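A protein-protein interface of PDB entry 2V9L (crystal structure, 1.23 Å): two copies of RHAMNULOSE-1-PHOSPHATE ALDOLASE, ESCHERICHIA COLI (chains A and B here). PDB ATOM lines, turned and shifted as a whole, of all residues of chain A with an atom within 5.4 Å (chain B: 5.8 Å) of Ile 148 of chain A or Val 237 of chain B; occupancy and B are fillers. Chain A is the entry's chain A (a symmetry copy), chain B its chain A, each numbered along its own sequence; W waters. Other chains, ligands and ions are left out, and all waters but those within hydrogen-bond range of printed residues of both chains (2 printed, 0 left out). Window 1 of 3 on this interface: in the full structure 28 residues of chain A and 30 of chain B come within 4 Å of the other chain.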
ATOM      1  N   HIS A 143     -29.899  27.408  12.281  1.00  0.00           N
ATOM      2  CA  HIS A 143     -28.972  26.456  11.741  1.00  0.00           C
ATOM      3  C   HIS A 143     -28.109  27.121  10.664  1.00  0.00           C
ATOM      4  O   HIS A 143     -28.174  26.870   9.469  1.00  0.00           O
ATOM      5  CB  HIS A 143     -29.720  25.200  11.203  1.00  0.00           C
ATOM      6  CG  HIS A 143     -30.406  24.478  12.313  1.00  0.00           C
ATOM      7  ND1 HIS A 143     -31.168  23.358  12.068  1.00  0.00           N
ATOM      8  CD2 HIS A 143     -30.460  24.671  13.656  1.00  0.00           C
ATOM      9  CE1 HIS A 143     -31.652  22.891  13.228  1.00  0.00           C
ATOM     10  NE2 HIS A 143     -31.261  23.677  14.231  1.00  0.00           N
ATOM     11  N   ALA A 144     -27.292  28.071  11.125  1.00  0.00           N
ATOM     12  CA  ALA A 144     -26.490  28.915  10.243  1.00  0.00           C
ATOM     13  C   ALA A 144     -25.446  28.058   9.543  1.00  0.00           C
ATOM     14  O   ALA A 144     -24.534  27.493  10.155  1.00  0.00           O
ATOM     15  CB  ALA A 144     -25.815  30.005  11.103  1.00  0.00           C
ATOM     16  N   THR A 145     -25.580  27.980   8.220  1.00  0.00           N
ATOM     17  CA  THR A 145     -24.918  26.951   7.403  1.00  0.00           C
ATOM     18  C   THR A 145     -23.430  26.916   7.511  1.00  0.00           C
ATOM     19  O   THR A 145     -22.831  25.826   7.720  1.00  0.00           O
ATOM     20  CB  THR A 145     -25.348  27.167   5.933  1.00  0.00           C
ATOM     21  OG1 THR A 145     -26.783  27.329   5.935  1.00  0.00           O
ATOM     22  CG2 THR A 145     -24.915  26.021   5.052  1.00  0.00           C
ATOM     23  N   ASN A 146     -22.761  28.050   7.264  1.00  0.00           N
ATOM     24  CA  ASN A 146     -21.311  28.088   7.298  1.00  0.00           C
ATOM     25  C   ASN A 146     -20.734  27.908   8.696  1.00  0.00           C
ATOM     26  O   ASN A 146     -19.739  27.226   8.845  1.00  0.00           O
ATOM     27  CB  ASN A 146     -20.794  29.360   6.610  1.00  0.00           C
ATOM     28  CG  ASN A 146     -21.092  29.290   5.128  1.00  0.00           C
ATOM     29  OD1 ASN A 146     -20.401  28.621   4.380  1.00  0.00           O
ATOM     30  ND2 ASN A 146     -22.124  30.024   4.728  1.00  0.00           N
ATOM     31  N   LEU A 147     -21.382  28.483   9.696  1.00  0.00           N
ATOM     32  CA  LEU A 147     -20.960  28.218  11.083  1.00  0.00           C
ATOM     33  C   LEU A 147     -21.022  26.735  11.377  1.00  0.00           C
ATOM     34  O   LEU A 147     -20.093  26.188  11.993  1.00  0.00           O
ATOM     35  CB  LEU A 147     -21.788  29.002  12.059  1.00  0.00           C
ATOM     36  CG  LEU A 147     -21.450  30.497  12.154  1.00  0.00           C
ATOM     37  CD1 LEU A 147     -22.579  31.269  12.840  1.00  0.00           C
ATOM     38  CD2 LEU A 147     -20.124  30.756  12.837  1.00  0.00           C
ATOM     39  N   ILE A 148     -22.084  26.042  10.953  1.00  0.00           N
ATOM     40  CA  ILE A 148     -22.174  24.608  11.153  1.00  0.00           C
ATOM     41  C   ILE A 148     -21.010  23.911  10.471  1.00  0.00           C
ATOM     42  O   ILE A 148     -20.320  23.071  11.054  1.00  0.00           O
ATOM     43  CB  ILE A 148     -23.528  24.063  10.666  1.00  0.00           C
ATOM     44  CG1 ILE A 148     -24.683  24.571  11.506  1.00  0.00           C
ATOM     45  CG2 ILE A 148     -23.484  22.538  10.642  1.00  0.00           C
ATOM     46  CD1 ILE A 148     -26.035  24.386  10.877  1.00  0.00           C
ATOM     47  N   ALA A 149     -20.777  24.224   9.197  1.00  0.00           N
ATOM     48  CA  ALA A 149     -19.687  23.571   8.458  1.00  0.00           C
ATOM     49  C   ALA A 149     -18.344  23.728   9.170  1.00  0.00           C
ATOM     50  O   ALA A 149     -17.546  22.806   9.242  1.00  0.00           O
ATOM     51  CB  ALA A 149     -19.619  24.079   7.033  1.00  0.00           C
ATOM     52  N   LEU A 150     -18.111  24.944   9.692  1.00  0.00           N
ATOM     53  CA  LEU A 150     -16.822  25.175  10.366  1.00  0.00           C
ATOM     54  C   LEU A 150     -16.663  24.319  11.606  1.00  0.00           C
ATOM     55  O   LEU A 150     -15.505  24.023  11.984  1.00  0.00           O
ATOM     56  CB  LEU A 150     -16.665  26.664  10.722  1.00  0.00           C
ATOM     57  CG  LEU A 150     -16.444  27.599   9.542  1.00  0.00           C
ATOM     58  CD1 LEU A 150     -16.279  29.032  10.004  1.00  0.00           C
ATOM     59  CD2 LEU A 150     -15.242  27.188   8.678  1.00  0.00           C
ATOM     60  N   THR A 151     -17.722  23.910  12.269  1.00  0.00           N
ATOM     61  CA  THR A 151     -17.582  23.080  13.447  1.00  0.00           C
ATOM     62  C   THR A 151     -17.014  21.690  13.126  1.00  0.00           C
ATOM     63  O   THR A 151     -16.580  20.997  14.058  1.00  0.00           O
ATOM     64  CB  THR A 151     -18.861  22.971  14.278  1.00  0.00           C
ATOM     65  OG1 THR A 151     -19.912  22.240  13.615  1.00  0.00           O
ATOM     66  CG2 THR A 151     -19.370  24.317  14.720  1.00  0.00           C
ATOM     67  N   TYR A 152     -16.992  21.280  11.869  1.00  0.00           N
ATOM     68  CA  TYR A 152     -16.352  20.010  11.474  1.00  0.00           C
ATOM     69  C   TYR A 152     -14.876  20.179  11.168  1.00  0.00           C
ATOM     70  O   TYR A 152     -14.195  19.142  11.061  1.00  0.00           O
ATOM     71  CB  TYR A 152     -17.020  19.342  10.264  1.00  0.00           C
ATOM     72  CG  TYR A 152     -18.491  19.058  10.476  1.00  0.00           C
ATOM     73  CD1 TYR A 152     -19.463  20.048  10.366  1.00  0.00           C
ATOM     74  CD2 TYR A 152     -18.942  17.787  10.812  1.00  0.00           C
ATOM     75  CE1 TYR A 152     -20.809  19.788  10.568  1.00  0.00           C
ATOM     76  CE2 TYR A 152     -20.277  17.513  11.029  1.00  0.00           C
ATOM     77  CZ  TYR A 152     -21.225  18.499  10.913  1.00  0.00           C
ATOM     78  OH  TYR A 152     -22.567  18.336  11.118  1.00  0.00           O
ATOM     79  N   PHE A 211     -22.032  20.855  15.068  1.00  0.00           N
ATOM     80  CA  PHE A 211     -22.761  19.914  14.214  1.00  0.00           C
ATOM     81  C   PHE A 211     -24.251  20.213  14.278  1.00  0.00           C
ATOM     82  O   PHE A 211     -25.084  19.348  13.936  1.00  0.00           O
ATOM     83  CB  PHE A 211     -22.463  18.442  14.549  1.00  0.00           C
ATOM     84  CG  PHE A 211     -21.048  18.182  14.980  1.00  0.00           C
ATOM     85  CD1 PHE A 211     -20.839  17.467  16.163  1.00  0.00           C
ATOM     86  CD2 PHE A 211     -19.963  18.633  14.273  1.00  0.00           C
ATOM     87  CE1 PHE A 211     -19.525  17.202  16.598  1.00  0.00           C
ATOM     88  CE2 PHE A 211     -18.663  18.402  14.707  1.00  0.00           C
ATOM     89  CZ  PHE A 211     -18.466  17.705  15.890  1.00  0.00           C
ATOM     90  N   HIS A 212     -24.629  21.437  14.669  1.00  0.00           N
ATOM     91  CA  HIS A 212     -26.021  21.783  14.928  1.00  0.00           C
ATOM     92  C   HIS A 212     -26.291  23.237  14.560  1.00  0.00           C
ATOM     93  O   HIS A 212     -27.121  23.514  13.680  1.00  0.00           O
ATOM     94  CB  HIS A 212     -26.421  21.377  16.363  1.00  0.00           C
ATOM     95  CG  HIS A 212     -27.888  21.584  16.629  1.00  0.00           C
ATOM     96  ND1 HIS A 212     -28.569  20.902  17.635  1.00  0.00           N
ATOM     97  CD2 HIS A 212     -28.872  22.374  16.133  1.00  0.00           C
ATOM     98  CE1 HIS A 212     -29.823  21.322  17.678  1.00  0.00           C
ATOM     99  NE2 HIS A 212     -30.082  22.256  16.725  1.00  0.00           N
ATOM    100  N   GLY A 213     -25.768  24.209  15.302  1.00  0.00           N
ATOM    101  CA  GLY A 213     -26.125  25.591  14.970  1.00  0.00           C
ATOM    102  C   GLY A 213     -25.581  26.571  15.997  1.00  0.00           C
ATOM    103  O   GLY A 213     -24.589  26.319  16.648  1.00  0.00           O
ATOM    104  N   GLU A 232     -22.131  34.602  10.770  1.00  0.00           N
ATOM    105  CA  GLU A 232     -22.319  33.696   9.649  1.00  0.00           C
ATOM    106  C   GLU A 232     -21.704  34.221   8.362  1.00  0.00           C
ATOM    107  O   GLU A 232     -21.251  33.419   7.540  1.00  0.00           O
ATOM    108  CB  GLU A 232     -23.832  33.437   9.510  1.00  0.00           C
ATOM    109  CG  GLU A 232     -24.241  32.630   8.281  1.00  0.00           C
ATOM    110  CD  GLU A 232     -23.658  31.227   8.150  1.00  0.00           C
ATOM    111  OE1 GLU A 232     -23.801  30.656   7.029  1.00  0.00           O
ATOM    112  OE2 GLU A 232     -23.115  30.685   9.137  1.00  0.00           O
ATOM    113  N   GLY B 168     -24.044  15.246   9.104  1.00  0.00           N
ATOM    114  CA  GLY B 168     -24.007  16.593   8.561  1.00  0.00           C
ATOM    115  C   GLY B 168     -25.015  17.579   9.101  1.00  0.00           C
ATOM    116  O   GLY B 168     -24.946  18.762   8.733  1.00  0.00           O
ATOM    117  N   SER B 169     -25.927  17.142   9.969  1.00  0.00           N
ATOM    118  CA  SER B 169     -26.755  18.041  10.778  1.00  0.00           C
ATOM    119  C   SER B 169     -27.407  17.167  11.864  1.00  0.00           C
ATOM    120  O   SER B 169     -27.979  16.115  11.553  1.00  0.00           O
ATOM    121  CB  SER B 169     -27.865  18.769  10.001  1.00  0.00           C
ATOM    122  OG  SER B 169     -27.330  19.788   9.141  1.00  0.00           O
ATOM    123  N   GLU B 232     -31.089  17.781   2.193  1.00  0.00           N
ATOM    124  CA  GLU B 232     -30.318  18.643   1.313  1.00  0.00           C
ATOM    125  C   GLU B 232     -29.488  19.664   2.074  1.00  0.00           C
ATOM    126  O   GLU B 232     -28.407  20.030   1.607  1.00  0.00           O
ATOM    127  CB  GLU B 232     -31.303  19.307   0.331  1.00  0.00           C
ATOM    128  CG  GLU B 232     -30.696  20.376  -0.573  1.00  0.00           C
ATOM    129  CD  GLU B 232     -29.563  19.939  -1.496  1.00  0.00           C
ATOM    130  OE1 GLU B 232     -28.905  20.860  -2.062  1.00  0.00           O
ATOM    131  OE2 GLU B 232     -29.357  18.722  -1.692  1.00  0.00           O
ATOM    132  N   LYS B 233     -29.976  20.122   3.223  1.00  0.00           N
ATOM    133  CA  LYS B 233     -29.212  21.005   4.074  1.00  0.00           C
ATOM    134  C   LYS B 233     -27.958  20.302   4.591  1.00  0.00           C
ATOM    135  O   LYS B 233     -26.853  20.841   4.594  1.00  0.00           O
ATOM    136  CB  LYS B 233     -30.053  21.520   5.228  1.00  0.00           C
ATOM    137  CG  LYS B 233     -29.317  22.301   6.290  1.00  0.00           C
ATOM    138  CD  LYS B 233     -28.646  23.585   5.802  1.00  0.00           C
ATOM    139  CE  LYS B 233     -28.191  24.472   6.924  1.00  0.00           C
ATOM    140  NZ  LYS B 233     -29.298  25.299   7.492  1.00  0.00           N
ATOM    141  N   SER B 234     -28.162  19.092   5.101  1.00  0.00           N
ATOM    142  CA  SER B 234     -27.002  18.306   5.515  1.00  0.00           C
ATOM    143  C   SER B 234     -26.043  18.105   4.361  1.00  0.00           C
ATOM    144  O   SER B 234     -24.823  18.262   4.525  1.00  0.00           O
ATOM    145  CB  SER B 234     -27.535  16.962   6.073  1.00  0.00           C
ATOM    146  OG  SER B 234     -26.362  16.247   6.488  1.00  0.00           O
ATOM    147  N   ALA B 235     -26.570  17.751   3.190  1.00  0.00           N
ATOM    148  CA  ALA B 235     -25.710  17.626   2.009  1.00  0.00           C
ATOM    149  C   ALA B 235     -24.936  18.896   1.694  1.00  0.00           C
ATOM    150  O   ALA B 235     -23.770  18.833   1.350  1.00  0.00           O
ATOM    151  CB  ALA B 235     -26.510  17.159   0.806  1.00  0.00           C
ATOM    152  N   GLN B 236     -25.569  20.064   1.849  1.00  0.00           N
ATOM    153  CA  GLN B 236     -24.903  21.336   1.623  1.00  0.00           C
ATOM    154  C   GLN B 236     -23.736  21.533   2.564  1.00  0.00           C
ATOM    155  O   GLN B 236     -22.644  21.976   2.170  1.00  0.00           O
ATOM    156  CB  GLN B 236     -25.938  22.455   1.754  1.00  0.00           C
ATOM    157  CG  GLN B 236     -25.368  23.829   1.493  1.00  0.00           C
ATOM    158  CD  GLN B 236     -26.309  24.947   1.730  1.00  0.00           C
ATOM    159  OE1 GLN B 236     -27.360  24.784   2.378  1.00  0.00           O
ATOM    160  NE2 GLN B 236     -25.951  26.114   1.259  1.00  0.00           N
ATOM    161  N   VAL B 237     -23.972  21.232   3.857  1.00  0.00           N
ATOM    162  CA  VAL B 237     -22.928  21.290   4.869  1.00  0.00           C
ATOM    163  C   VAL B 237     -21.799  20.342   4.492  1.00  0.00           C
ATOM    164  O   VAL B 237     -20.611  20.721   4.530  1.00  0.00           O
ATOM    165  CB  VAL B 237     -23.505  20.976   6.270  1.00  0.00           C
ATOM    166  CG1 VAL B 237     -22.389  20.763   7.266  1.00  0.00           C
ATOM    167  CG2 VAL B 237     -24.443  22.085   6.727  1.00  0.00           C
ATOM    168  N   LEU B 238     -22.116  19.104   4.138  1.00  0.00           N
ATOM    169  CA  LEU B 238     -21.104  18.119   3.769  1.00  0.00           C
ATOM    170  C   LEU B 238     -20.282  18.582   2.579  1.00  0.00           C
ATOM    171  O   LEU B 238     -19.046  18.431   2.585  1.00  0.00           O
ATOM    172  CB  LEU B 238     -21.758  16.764   3.468  1.00  0.00           C
ATOM    173  CG  LEU B 238     -22.385  16.049   4.673  1.00  0.00           C
ATOM    174  CD1 LEU B 238     -23.082  14.786   4.141  1.00  0.00           C
ATOM    175  CD2 LEU B 238     -21.401  15.689   5.744  1.00  0.00           C
ATOM    176  N   VAL B 239     -20.907  19.140   1.544  1.00  0.00           N
ATOM    177  CA  VAL B 239     -20.146  19.611   0.386  1.00  0.00           C
ATOM    178  C   VAL B 239     -19.137  20.665   0.819  1.00  0.00           C
ATOM    179  O   VAL B 239     -17.982  20.661   0.373  1.00  0.00           O
ATOM    180  CB  VAL B 239     -21.074  20.086  -0.731  1.00  0.00           C
ATOM    181  CG1 VAL B 239     -20.320  20.822  -1.833  1.00  0.00           C
ATOM    182  CG2 VAL B 239     -21.828  18.895  -1.341  1.00  0.00           C
ATOM    183  N   LYS B 240     -19.539  21.593   1.701  1.00  0.00           N
ATOM    184  CA  LYS B 240     -18.593  22.581   2.239  1.00  0.00           C
ATOM    185  C   LYS B 240     -17.451  21.881   2.979  1.00  0.00           C
ATOM    186  O   LYS B 240     -16.292  22.192   2.762  1.00  0.00           O
ATOM    187  CB  LYS B 240     -19.287  23.583   3.161  1.00  0.00           C
ATOM    188  CG  LYS B 240     -20.224  24.536   2.435  1.00  0.00           C
ATOM    189  CD  LYS B 240     -21.023  25.412   3.385  1.00  0.00           C
ATOM    190  CE  LYS B 240     -21.978  26.358   2.723  1.00  0.00           C
ATOM    191  NZ  LYS B 240     -21.247  27.462   2.036  1.00  0.00           N
ATOM    192  N   VAL B 241     -17.783  20.979   3.885  1.00  0.00           N
ATOM    193  CA  VAL B 241     -16.758  20.300   4.702  1.00  0.00           C
ATOM    194  C   VAL B 241     -15.786  19.522   3.842  1.00  0.00           C
ATOM    195  O   VAL B 241     -14.567  19.623   4.005  1.00  0.00           O
ATOM    196  CB  VAL B 241     -17.449  19.427   5.759  1.00  0.00           C
ATOM    197  CG1 VAL B 241     -16.424  18.522   6.478  1.00  0.00           C
ATOM    198  CG2 VAL B 241     -18.199  20.263   6.783  1.00  0.00           C
ATOM    199  N   TYR B 242     -16.336  18.755   2.874  1.00  0.00           N
ATOM    200  CA  TYR B 242     -15.459  17.993   1.993  1.00  0.00           C
ATOM    201  C   TYR B 242     -14.581  18.887   1.153  1.00  0.00           C
ATOM    202  O   TYR B 242     -13.401  18.607   0.939  1.00  0.00           O
ATOM    203  CB  TYR B 242     -16.287  17.066   1.088  1.00  0.00           C
ATOM    204  CG  TYR B 242     -17.119  16.002   1.817  1.00  0.00           C
ATOM    205  CD1 TYR B 242     -18.263  15.538   1.200  1.00  0.00           C
ATOM    206  CD2 TYR B 242     -16.829  15.477   3.045  1.00  0.00           C
ATOM    207  CE1 TYR B 242     -19.090  14.587   1.757  1.00  0.00           C
ATOM    208  CE2 TYR B 242     -17.641  14.524   3.643  1.00  0.00           C
ATOM    209  CZ  TYR B 242     -18.731  14.103   3.021  1.00  0.00           C
ATOM    210  OH  TYR B 242     -19.647  13.178   3.417  1.00  0.00           O
HETATM  211  O   HOH W   1     -23.005  29.696   1.856  1.00  0.00           O
HETATM  212  O   HOH W   2     -18.938  29.830   1.660  1.00  0.00           O
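The backbone carbonyl oxygen (O) of Gly 168 of chain B lies close to the side-chain hydroxyl (OH) of Tyr 152 of chain A, 3.4 Å away.
NZ of Lys 233 of chain B is in hydrogen-bond range of O of His 143 of chain A, 2.8 Å away.
The side-chain amide oxygen of Asn 146 of chain A sits at hydrogen-bond distance from the side-chain amino group of Lys 240 of chain B (2.7 Å).
The backbone carbonyl oxygen of Ile 148 of chain A is in hydrogen-bond range of the side-chain hydroxyl of Thr 151 of chain A (2.7 Å).
The side-chain carboxylate (OE1) of Glu 232 of chain A lies within hydrogen-bond range of the backbone NH (N) of Thr 145 of chain A (3.4 Å).
The side-chain carboxylate of Glu 232 of chain A sits at hydrogen-bond distance from the backbone NH of Asn 146 of chain A (2.8 Å).
The side-chain hydroxyl (OG1) of Thr 151 of chain A sits at hydrogen-bond distance from the backbone NH (N) of Phe 211 of chain A, 2.9 Å away.
Among the printed residues, merely in contact across the chains: Thr 145 of chain A with Lys 233 of chain B, Ala 149 of chain A with Val 241 of chain B, Tyr 152 of chain A with Ser 169 of chain B, Thr 145 of chain A with Gln 236 of chain B, Thr 145 of chain A with Lys 240 of chain B, Tyr 152 of chain A with Val 237 of chain B, Tyr 152 of chain A with Val 241 of chain B, Phe 211 of chain A with Ser 169 of chain B, Ala 149 of chain A with Lys 240 of chain B and Ile 148 of chain A with Val 237 of chain B.
Ile 148 of chain A touches one residue of chain B.
Val 237 of chain B touches just these residues of chain A: Ile 148 (3.97 Å) and Tyr 152 (3.8 Å).
Of the printed residues of chain A, Ser 169 of chain B touches Tyr 152 and Phe 211.
Printed residues of chain A within 4 Å of Gly 168 of chain B: Tyr 152.
The nearest residue of chain A that does not touch Val 237 of chain B is Ala 149 of chain A (4.1 Å).
Hydrophobic or aromatic side chains of chain B within 4 Å of the printed part of chain A: Val 237 and Val 241.
Printed residues of chain A that touch a printed residue of chain B: His 143, Thr 145, Asn 146, Ile 148, Ala 149, Tyr 152 and Phe 211.
Hydrophobic or aromatic side chains of chain A that line the printed part of chain B: His 143, Ile 148, Ala 149 and Tyr 152.
Among the printed residues, no Asp or Glu carboxylate lies within 4 Å of a Lys or Arg side-chain nitrogen of the other chain.
1 position is printed for both chains.
Water W1 lies within hydrogen-bond range of the side-chain amino group of Lys 240 of chain B and the side-chain amide nitrogen of Asn 146 of chain A.
Water W2 bridges OD1 of Asn 146 of chain A (3.3 Å) and NZ of Lys 240 of chain B (3.3 Å).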
